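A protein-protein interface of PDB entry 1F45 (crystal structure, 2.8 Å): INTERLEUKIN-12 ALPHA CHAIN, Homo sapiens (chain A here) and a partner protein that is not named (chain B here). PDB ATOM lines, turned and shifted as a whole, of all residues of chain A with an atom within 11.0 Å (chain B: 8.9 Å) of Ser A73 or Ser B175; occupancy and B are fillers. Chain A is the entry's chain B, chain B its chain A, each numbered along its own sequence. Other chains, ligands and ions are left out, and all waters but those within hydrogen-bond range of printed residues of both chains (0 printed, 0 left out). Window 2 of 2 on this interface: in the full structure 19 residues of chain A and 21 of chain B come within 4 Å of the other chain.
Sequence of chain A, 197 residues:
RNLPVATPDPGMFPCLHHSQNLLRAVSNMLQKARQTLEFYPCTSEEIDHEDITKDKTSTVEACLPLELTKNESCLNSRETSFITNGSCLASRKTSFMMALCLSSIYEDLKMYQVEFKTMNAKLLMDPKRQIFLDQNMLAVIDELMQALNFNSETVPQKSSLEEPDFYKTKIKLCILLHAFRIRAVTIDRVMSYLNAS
Glu A61 touches none of the printed residues of chain B.
Of the printed residues of chain B, Leu A64 touches Ala B179.
Ser A73 touches just these residues of chain B: Ser B175 (3.4 Å), Ala B176 (3.7 Å) and Cys B177 (3.3 Å).
Of chain B, only Cys B177 and Pro B178 come within 4 Å of Cys A74.
No residue of chain A comes within 4 Å of Glu B173.
Of the printed residues of chain A, Ser B175 touches Ser A73 (3.4 Å).
Of the printed residues of chain A, Ala B176 touches Ser A73.
Cys B177 touches just these residues of chain A: Ser A73 and Cys A74.
Of the printed residues of chain A, Pro B178 touches Cys A74 (3.7 Å).
Printed residues of chain A within 4 Å of Ala B179: Val A60 (3.4 Å), Leu A64 (3.8 Å) and Leu A68 (3.4 Å).
The nearest residue of chain A that does not touch Ser B175 is Glu A72 (5.8 Å).
The nearest printed residue of chain B that does not touch Val A60 is Ala B180 (4.6 Å).
Among the printed residues, pairs that only touch across the chains: Val A60 with Ala B179 (3.4 Å), Leu A64 with Ala B179 (3.8 Å), Leu A68 with Ala B179 (3.4 Å), Ser A73 with Ser B175 (3.4 Å), Ser A73 with Ala B176 (3.7 Å), Ser A73 with Cys B177 (3.3 Å) and Cys A74 with Pro B178 (3.7 Å).
Hydrophobic or aromatic side chains of chain A within 4 Å of the printed part of chain B: Val A60, Leu A64 and Leu A68.
Along chain A the printed residues that touch a printed residue of chain B span positions 60 to 74.
Among the printed residues, no Asp or Glu carboxylate lies within 4 Å of a Lys or Arg side-chain nitrogen of the other chain.
The side-chain amide nitrogen (ND2) of Asn A71 is in hydrogen-bond range of the side-chain hydroxyl (OG) of Ser A73, 2.9 Å away.
SG of Cys B177 lies close to N of Ala B179 (3.5 Å).
SG of Cys B177 is disulfide-bonded to SG of Cys A74 (2.1 Å).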
ATOM      1  N   VAL A  60      12.862   1.515 -20.716  1.00  0.00           N
ATOM      2  CA  VAL A  60      13.275   0.498 -19.768  1.00  0.00           C
ATOM      3  C   VAL A  60      12.152   0.014 -18.876  1.00  0.00           C
ATOM      4  O   VAL A  60      12.079  -1.167 -18.569  1.00  0.00           O
ATOM      5  CB  VAL A  60      14.395   0.993 -18.805  1.00  0.00           C
ATOM      6  CG1 VAL A  60      14.589  -0.004 -17.716  1.00  0.00           C
ATOM      7  CG2 VAL A  60      15.646   1.166 -19.518  1.00  0.00           C
ATOM      8  N   GLU A  61      11.304   0.925 -18.427  1.00  0.00           N
ATOM      9  CA  GLU A  61      10.225   0.544 -17.518  1.00  0.00           C
ATOM     10  C   GLU A  61       9.031   0.115 -18.312  1.00  0.00           C
ATOM     11  O   GLU A  61       8.446  -0.928 -18.071  1.00  0.00           O
ATOM     12  CB  GLU A  61       9.844   1.709 -16.633  1.00  0.00           C
ATOM     13  CG  GLU A  61      10.985   2.613 -16.346  1.00  0.00           C
ATOM     14  CD  GLU A  61      10.590   3.805 -15.472  1.00  0.00           C
ATOM     15  OE1 GLU A  61       9.644   4.562 -15.865  1.00  0.00           O
ATOM     16  OE2 GLU A  61      11.249   3.974 -14.399  1.00  0.00           O
ATOM     17  N   LEU A  64       9.517  -3.175 -18.836  1.00  0.00           N
ATOM     18  CA  LEU A  64      10.145  -3.922 -17.774  1.00  0.00           C
ATOM     19  C   LEU A  64       9.558  -5.342 -17.694  1.00  0.00           C
ATOM     20  O   LEU A  64       8.346  -5.539 -17.781  1.00  0.00           O
ATOM     21  CB  LEU A  64       9.970  -3.221 -16.452  1.00  0.00           C
ATOM     22  CG  LEU A  64      10.759  -3.992 -15.409  1.00  0.00           C
ATOM     23  CD1 LEU A  64      12.243  -3.741 -15.591  1.00  0.00           C
ATOM     24  CD2 LEU A  64      10.340  -3.532 -14.055  1.00  0.00           C
ATOM     25  N   PRO A  65      10.418  -6.359 -17.562  1.00  0.00           N
ATOM     26  CA  PRO A  65       9.951  -7.751 -17.485  1.00  0.00           C
ATOM     27  C   PRO A  65       9.126  -7.991 -16.240  1.00  0.00           C
ATOM     28  O   PRO A  65       9.440  -7.439 -15.206  1.00  0.00           O
ATOM     29  CB  PRO A  65      11.260  -8.553 -17.476  1.00  0.00           C
ATOM     30  CG  PRO A  65      12.124  -7.693 -18.314  1.00  0.00           C
ATOM     31  CD  PRO A  65      11.868  -6.311 -17.783  1.00  0.00           C
ATOM     32  N   GLU A  67       8.957 -10.402 -14.149  1.00  0.00           N
ATOM     33  CA  GLU A  67       9.746 -10.809 -13.036  1.00  0.00           C
ATOM     34  C   GLU A  67      10.496  -9.737 -12.312  1.00  0.00           C
ATOM     35  O   GLU A  67      10.628  -9.838 -11.096  1.00  0.00           O
ATOM     36  CB  GLU A  67      10.711 -11.895 -13.439  1.00  0.00           C
ATOM     37  CG  GLU A  67      11.081 -11.799 -14.859  1.00  0.00           C
ATOM     38  CD  GLU A  67      10.054 -12.397 -15.783  1.00  0.00           C
ATOM     39  OE1 GLU A  67       9.911 -13.631 -15.765  1.00  0.00           O
ATOM     40  OE2 GLU A  67       9.414 -11.634 -16.525  1.00  0.00           O
ATOM     41  N   LEU A  68      11.003  -8.723 -13.012  1.00  0.00           N
ATOM     42  CA  LEU A  68      11.763  -7.658 -12.317  1.00  0.00           C
ATOM     43  C   LEU A  68      10.889  -6.767 -11.415  1.00  0.00           C
ATOM     44  O   LEU A  68      11.369  -5.868 -10.712  1.00  0.00           O
ATOM     45  CB  LEU A  68      12.550  -6.778 -13.332  1.00  0.00           C
ATOM     46  CG  LEU A  68      13.833  -7.436 -13.893  1.00  0.00           C
ATOM     47  CD1 LEU A  68      14.610  -6.414 -14.675  1.00  0.00           C
ATOM     48  CD2 LEU A  68      14.721  -7.998 -12.779  1.00  0.00           C
ATOM     49  N   THR A  69       9.591  -7.029 -11.455  1.00  0.00           N
ATOM     50  CA  THR A  69       8.619  -6.310 -10.661  1.00  0.00           C
ATOM     51  C   THR A  69       8.730  -6.744  -9.184  1.00  0.00           C
ATOM     52  O   THR A  69       8.614  -5.935  -8.259  1.00  0.00           O
ATOM     53  CB  THR A  69       7.272  -6.606 -11.212  1.00  0.00           C
ATOM     54  OG1 THR A  69       7.149  -5.927 -12.463  1.00  0.00           O
ATOM     55  CG2 THR A  69       6.209  -6.144 -10.264  1.00  0.00           C
ATOM     56  N   LYS A  70       8.961  -8.032  -8.987  1.00  0.00           N
ATOM     57  CA  LYS A  70       9.142  -8.571  -7.672  1.00  0.00           C
ATOM     58  C   LYS A  70      10.266  -7.844  -6.930  1.00  0.00           C
ATOM     59  O   LYS A  70      10.437  -8.060  -5.734  1.00  0.00           O
ATOM     60  CB  LYS A  70       9.538 -10.033  -7.783  1.00  0.00           C
ATOM     61  CG  LYS A  70       8.710 -10.810  -8.786  1.00  0.00           C
ATOM     62  CD  LYS A  70       9.247 -12.250  -8.979  1.00  0.00           C
ATOM     63  CE  LYS A  70       8.318 -13.101  -9.893  1.00  0.00           C
ATOM     64  NZ  LYS A  70       8.844 -14.477 -10.165  1.00  0.00           N
ATOM     65  N   ASN A  71      11.045  -7.002  -7.613  1.00  0.00           N
ATOM     66  CA  ASN A  71      12.176  -6.315  -6.968  1.00  0.00           C
ATOM     67  C   ASN A  71      11.907  -4.853  -6.726  1.00  0.00           C
ATOM     68  O   ASN A  71      11.773  -4.064  -7.646  1.00  0.00           O
ATOM     69  CB  ASN A  71      13.446  -6.505  -7.804  1.00  0.00           C
ATOM     70  CG  ASN A  71      14.669  -5.788  -7.230  1.00  0.00           C
ATOM     71  OD1 ASN A  71      15.799  -6.121  -7.596  1.00  0.00           O
ATOM     72  ND2 ASN A  71      14.455  -4.785  -6.367  1.00  0.00           N
ATOM     73  N   GLU A  72      11.851  -4.532  -5.439  1.00  0.00           N
ATOM     74  CA  GLU A  72      11.570  -3.201  -4.907  1.00  0.00           C
ATOM     75  C   GLU A  72      11.879  -2.015  -5.808  1.00  0.00           C
ATOM     76  O   GLU A  72      10.995  -1.300  -6.302  1.00  0.00           O
ATOM     77  CB  GLU A  72      12.348  -3.028  -3.598  1.00  0.00           C
ATOM     78  CG  GLU A  72      11.492  -2.812  -2.309  1.00  0.00           C
ATOM     79  CD  GLU A  72      11.155  -4.117  -1.522  1.00  0.00           C
ATOM     80  OE1 GLU A  72       9.944  -4.429  -1.388  1.00  0.00           O
ATOM     81  OE2 GLU A  72      12.092  -4.814  -1.031  1.00  0.00           O
ATOM     82  N   SER A  73      13.174  -1.842  -6.001  1.00  0.00           N
ATOM     83  CA  SER A  73      13.789  -0.761  -6.761  1.00  0.00           C
ATOM     84  C   SER A  73      13.704  -0.644  -8.280  1.00  0.00           C
ATOM     85  O   SER A  73      14.528   0.063  -8.850  1.00  0.00           O
ATOM     86  CB  SER A  73      15.255  -0.763  -6.385  1.00  0.00           C
ATOM     87  OG  SER A  73      15.664  -2.126  -6.231  1.00  0.00           O
ATOM     88  N   CYS A  74      12.745  -1.271  -8.955  1.00  0.00           N
ATOM     89  CA  CYS A  74      12.740  -1.161 -10.415  1.00  0.00           C
ATOM     90  C   CYS A  74      11.728  -0.234 -11.121  1.00  0.00           C
ATOM     91  O   CYS A  74      10.553  -0.122 -10.760  1.00  0.00           O
ATOM     92  CB  CYS A  74      12.684  -2.562 -11.031  1.00  0.00           C
ATOM     93  SG  CYS A  74      14.271  -3.474 -11.149  1.00  0.00           S
ATOM     94  N   THR A  80       2.717   1.201 -12.796  1.00  0.00           N
ATOM     95  CA  THR A  80       3.504  -0.008 -12.524  1.00  0.00           C
ATOM     96  C   THR A  80       3.398  -1.119 -13.594  1.00  0.00           C
ATOM     97  O   THR A  80       3.060  -2.282 -13.313  1.00  0.00           O
ATOM     98  CB  THR A  80       3.143  -0.605 -11.135  1.00  0.00           C
ATOM     99  OG1 THR A  80       3.674  -1.935 -11.051  1.00  0.00           O
ATOM    100  CG2 THR A  80       1.611  -0.637 -10.911  1.00  0.00           C
ATOM    101  N   SER A  81       3.727  -0.738 -14.822  1.00  0.00           N
ATOM    102  CA  SER A  81       3.677  -1.619 -15.975  1.00  0.00           C
ATOM    103  C   SER A  81       4.737  -2.679 -16.157  1.00  0.00           C
ATOM    104  O   SER A  81       5.773  -2.697 -15.494  1.00  0.00           O
ATOM    105  CB  SER A  81       3.637  -0.781 -17.238  1.00  0.00           C
ATOM    106  OG  SER A  81       2.328  -0.280 -17.442  1.00  0.00           O
ATOM    107  N   SER B 115      23.529  -7.006 -10.486  1.00  0.00           N
ATOM    108  CA  SER B 115      22.900  -6.839  -9.178  1.00  0.00           C
ATOM    109  C   SER B 115      23.189  -5.528  -8.501  1.00  0.00           C
ATOM    110  O   SER B 115      22.386  -5.066  -7.706  1.00  0.00           O
ATOM    111  CB  SER B 115      23.319  -7.955  -8.233  1.00  0.00           C
ATOM    112  OG  SER B 115      24.681  -7.825  -7.891  1.00  0.00           O
ATOM    113  N   GLY B 116      24.341  -4.943  -8.811  1.00  0.00           N
ATOM    114  CA  GLY B 116      24.740  -3.690  -8.193  1.00  0.00           C
ATOM    115  C   GLY B 116      25.787  -3.960  -7.127  1.00  0.00           C
ATOM    116  O   GLY B 116      26.310  -3.043  -6.480  1.00  0.00           O
ATOM    117  N   ARG B 138      27.531   6.614  -6.640  1.00  0.00           N
ATOM    118  CA  ARG B 138      27.322   6.693  -8.067  1.00  0.00           C
ATOM    119  C   ARG B 138      27.019   8.113  -8.443  1.00  0.00           C
ATOM    120  O   ARG B 138      25.997   8.660  -8.071  1.00  0.00           O
ATOM    121  CB  ARG B 138      26.203   5.792  -8.534  1.00  0.00           C
ATOM    122  CG  ARG B 138      26.226   5.807 -10.060  1.00  0.00           C
ATOM    123  CD  ARG B 138      25.055   5.151 -10.717  1.00  0.00           C
ATOM    124  NE  ARG B 138      25.108   3.721 -10.557  1.00  0.00           N
ATOM    125  CZ  ARG B 138      25.576   2.898 -11.482  1.00  0.00           C
ATOM    126  NH1 ARG B 138      26.039   3.413 -12.626  1.00  0.00           N
ATOM    127  NH2 ARG B 138      25.535   1.562 -11.275  1.00  0.00           N
ATOM    128  N   GLN B 144      24.874   9.185  -5.412  1.00  0.00           N
ATOM    129  CA  GLN B 144      23.787   8.257  -5.079  1.00  0.00           C
ATOM    130  C   GLN B 144      24.477   7.186  -4.238  1.00  0.00           C
ATOM    131  O   GLN B 144      25.668   6.907  -4.421  1.00  0.00           O
ATOM    132  CB  GLN B 144      23.183   7.605  -6.329  1.00  0.00           C
ATOM    133  CG  GLN B 144      22.371   8.516  -7.256  1.00  0.00           C
ATOM    134  CD  GLN B 144      21.223   9.220  -6.540  1.00  0.00           C
ATOM    135  OE1 GLN B 144      21.409  10.278  -5.940  1.00  0.00           O
ATOM    136  NE2 GLN B 144      20.033   8.627  -6.595  1.00  0.00           N
ATOM    137  N   GLY B 145      23.728   6.552  -3.345  1.00  0.00           N
ATOM    138  CA  GLY B 145      24.330   5.588  -2.447  1.00  0.00           C
ATOM    139  C   GLY B 145      24.857   4.221  -2.794  1.00  0.00           C
ATOM    140  O   GLY B 145      24.212   3.427  -3.484  1.00  0.00           O
ATOM    141  N   VAL B 146      26.028   3.943  -2.236  1.00  0.00           N
ATOM    142  CA  VAL B 146      26.689   2.650  -2.388  1.00  0.00           C
ATOM    143  C   VAL B 146      27.159   2.256  -1.009  1.00  0.00           C
ATOM    144  O   VAL B 146      27.695   3.059  -0.288  1.00  0.00           O
ATOM    145  CB  VAL B 146      27.938   2.699  -3.295  1.00  0.00           C
ATOM    146  CG1 VAL B 146      28.644   1.328  -3.275  1.00  0.00           C
ATOM    147  CG2 VAL B 146      27.534   3.092  -4.681  1.00  0.00           C
ATOM    148  N   THR B 147      26.985   1.015  -0.630  1.00  0.00           N
ATOM    149  CA  THR B 147      27.409   0.658   0.690  1.00  0.00           C
ATOM    150  C   THR B 147      28.548  -0.352   0.612  1.00  0.00           C
ATOM    151  O   THR B 147      28.412  -1.438   0.000  1.00  0.00           O
ATOM    152  CB  THR B 147      26.196   0.125   1.469  1.00  0.00           C
ATOM    153  OG1 THR B 147      25.222   1.181   1.631  1.00  0.00           O
ATOM    154  CG2 THR B 147      26.627  -0.419   2.786  1.00  0.00           C
ATOM    155  N   GLN B 172      27.804  -2.709  -2.540  1.00  0.00           N
ATOM    156  CA  GLN B 172      26.499  -2.995  -3.130  1.00  0.00           C
ATOM    157  C   GLN B 172      25.815  -1.707  -3.494  1.00  0.00           C
ATOM    158  O   GLN B 172      25.600  -0.869  -2.621  1.00  0.00           O
ATOM    159  CB  GLN B 172      25.642  -3.747  -2.117  1.00  0.00           C
ATOM    160  CG  GLN B 172      24.172  -3.841  -2.428  1.00  0.00           C
ATOM    161  CD  GLN B 172      23.880  -4.648  -3.684  1.00  0.00           C
ATOM    162  OE1 GLN B 172      23.278  -4.139  -4.649  1.00  0.00           O
ATOM    163  NE2 GLN B 172      24.295  -5.908  -3.680  1.00  0.00           N
ATOM    164  N   GLU B 173      25.481  -1.510  -4.771  1.00  0.00           N
ATOM    165  CA  GLU B 173      24.794  -0.275  -5.075  1.00  0.00           C
ATOM    166  C   GLU B 173      23.495  -0.361  -4.296  1.00  0.00           C
ATOM    167  O   GLU B 173      22.891  -1.443  -4.215  1.00  0.00           O
ATOM    168  CB  GLU B 173      24.524  -0.129  -6.548  1.00  0.00           C
ATOM    169  CG  GLU B 173      24.194   1.264  -6.803  1.00  0.00           C
ATOM    170  CD  GLU B 173      23.959   1.533  -8.230  1.00  0.00           C
ATOM    171  OE1 GLU B 173      24.364   0.669  -9.047  1.00  0.00           O
ATOM    172  OE2 GLU B 173      23.393   2.619  -8.536  1.00  0.00           O
ATOM    173  N   ASP B 174      23.041   0.763  -3.740  1.00  0.00           N
ATOM    174  CA  ASP B 174      21.847   0.713  -2.896  1.00  0.00           C
ATOM    175  C   ASP B 174      20.442   0.444  -3.416  1.00  0.00           C
ATOM    176  O   ASP B 174      19.905  -0.647  -3.174  1.00  0.00           O
ATOM    177  CB  ASP B 174      21.833   1.905  -1.925  1.00  0.00           C
ATOM    178  CG  ASP B 174      22.781   1.679  -0.714  1.00  0.00           C
ATOM    179  OD1 ASP B 174      23.123   0.486  -0.395  1.00  0.00           O
ATOM    180  OD2 ASP B 174      23.171   2.693  -0.072  1.00  0.00           O
ATOM    181  N   SER B 175      19.798   1.379  -4.083  1.00  0.00           N
ATOM    182  CA  SER B 175      18.443   1.029  -4.540  1.00  0.00           C
ATOM    183  C   SER B 175      18.584   0.743  -6.028  1.00  0.00           C
ATOM    184  O   SER B 175      18.119   1.528  -6.879  1.00  0.00           O
ATOM    185  CB  SER B 175      17.453   2.183  -4.274  1.00  0.00           C
ATOM    186  OG  SER B 175      16.106   1.700  -4.227  1.00  0.00           O
ATOM    187  N   ALA B 176      19.219  -0.407  -6.294  1.00  0.00           N
ATOM    188  CA  ALA B 176      19.613  -0.886  -7.628  1.00  0.00           C
ATOM    189  C   ALA B 176      18.785  -1.815  -8.502  1.00  0.00           C
ATOM    190  O   ALA B 176      18.678  -3.027  -8.255  1.00  0.00           O
ATOM    191  CB  ALA B 176      21.028  -1.477  -7.519  1.00  0.00           C
ATOM    192  N   CYS B 177      18.259  -1.248  -9.575  1.00  0.00           N
ATOM    193  CA  CYS B 177      17.508  -2.042 -10.531  1.00  0.00           C
ATOM    194  C   CYS B 177      18.470  -2.593 -11.598  1.00  0.00           C
ATOM    195  O   CYS B 177      19.093  -1.842 -12.381  1.00  0.00           O
ATOM    196  CB  CYS B 177      16.436  -1.214 -11.220  1.00  0.00           C
ATOM    197  SG  CYS B 177      15.476  -2.284 -12.320  1.00  0.00           S
ATOM    198  N   PRO B 178      18.580  -3.922 -11.668  1.00  0.00           N
ATOM    199  CA  PRO B 178      19.461  -4.560 -12.648  1.00  0.00           C
ATOM    200  C   PRO B 178      19.125  -4.124 -14.063  1.00  0.00           C
ATOM    201  O   PRO B 178      20.003  -4.147 -14.904  1.00  0.00           O
ATOM    202  CB  PRO B 178      19.166  -6.037 -12.462  1.00  0.00           C
ATOM    203  CG  PRO B 178      18.530  -6.131 -11.104  1.00  0.00           C
ATOM    204  CD  PRO B 178      17.683  -4.915 -11.061  1.00  0.00           C
ATOM    205  N   ALA B 179      17.866  -3.746 -14.343  1.00  0.00           N
ATOM    206  CA  ALA B 179      17.472  -3.318 -15.694  1.00  0.00           C
ATOM    207  C   ALA B 179      17.731  -1.871 -16.064  1.00  0.00           C
ATOM    208  O   ALA B 179      17.568  -1.481 -17.199  1.00  0.00           O
ATOM    209  CB  ALA B 179      16.054  -3.642 -15.950  1.00  0.00           C
ATOM    210  N   ALA B 180      18.195  -1.094 -15.114  1.00  0.00           N
ATOM    211  CA  ALA B 180      18.509   0.305 -15.317  1.00  0.00           C
ATOM    212  C   ALA B 180      19.669   0.595 -16.267  1.00  0.00           C
ATOM    213  O   ALA B 180      20.738   0.082 -16.080  1.00  0.00           O
ATOM    214  CB  ALA B 180      18.837   0.889 -14.001  1.00  0.00           C
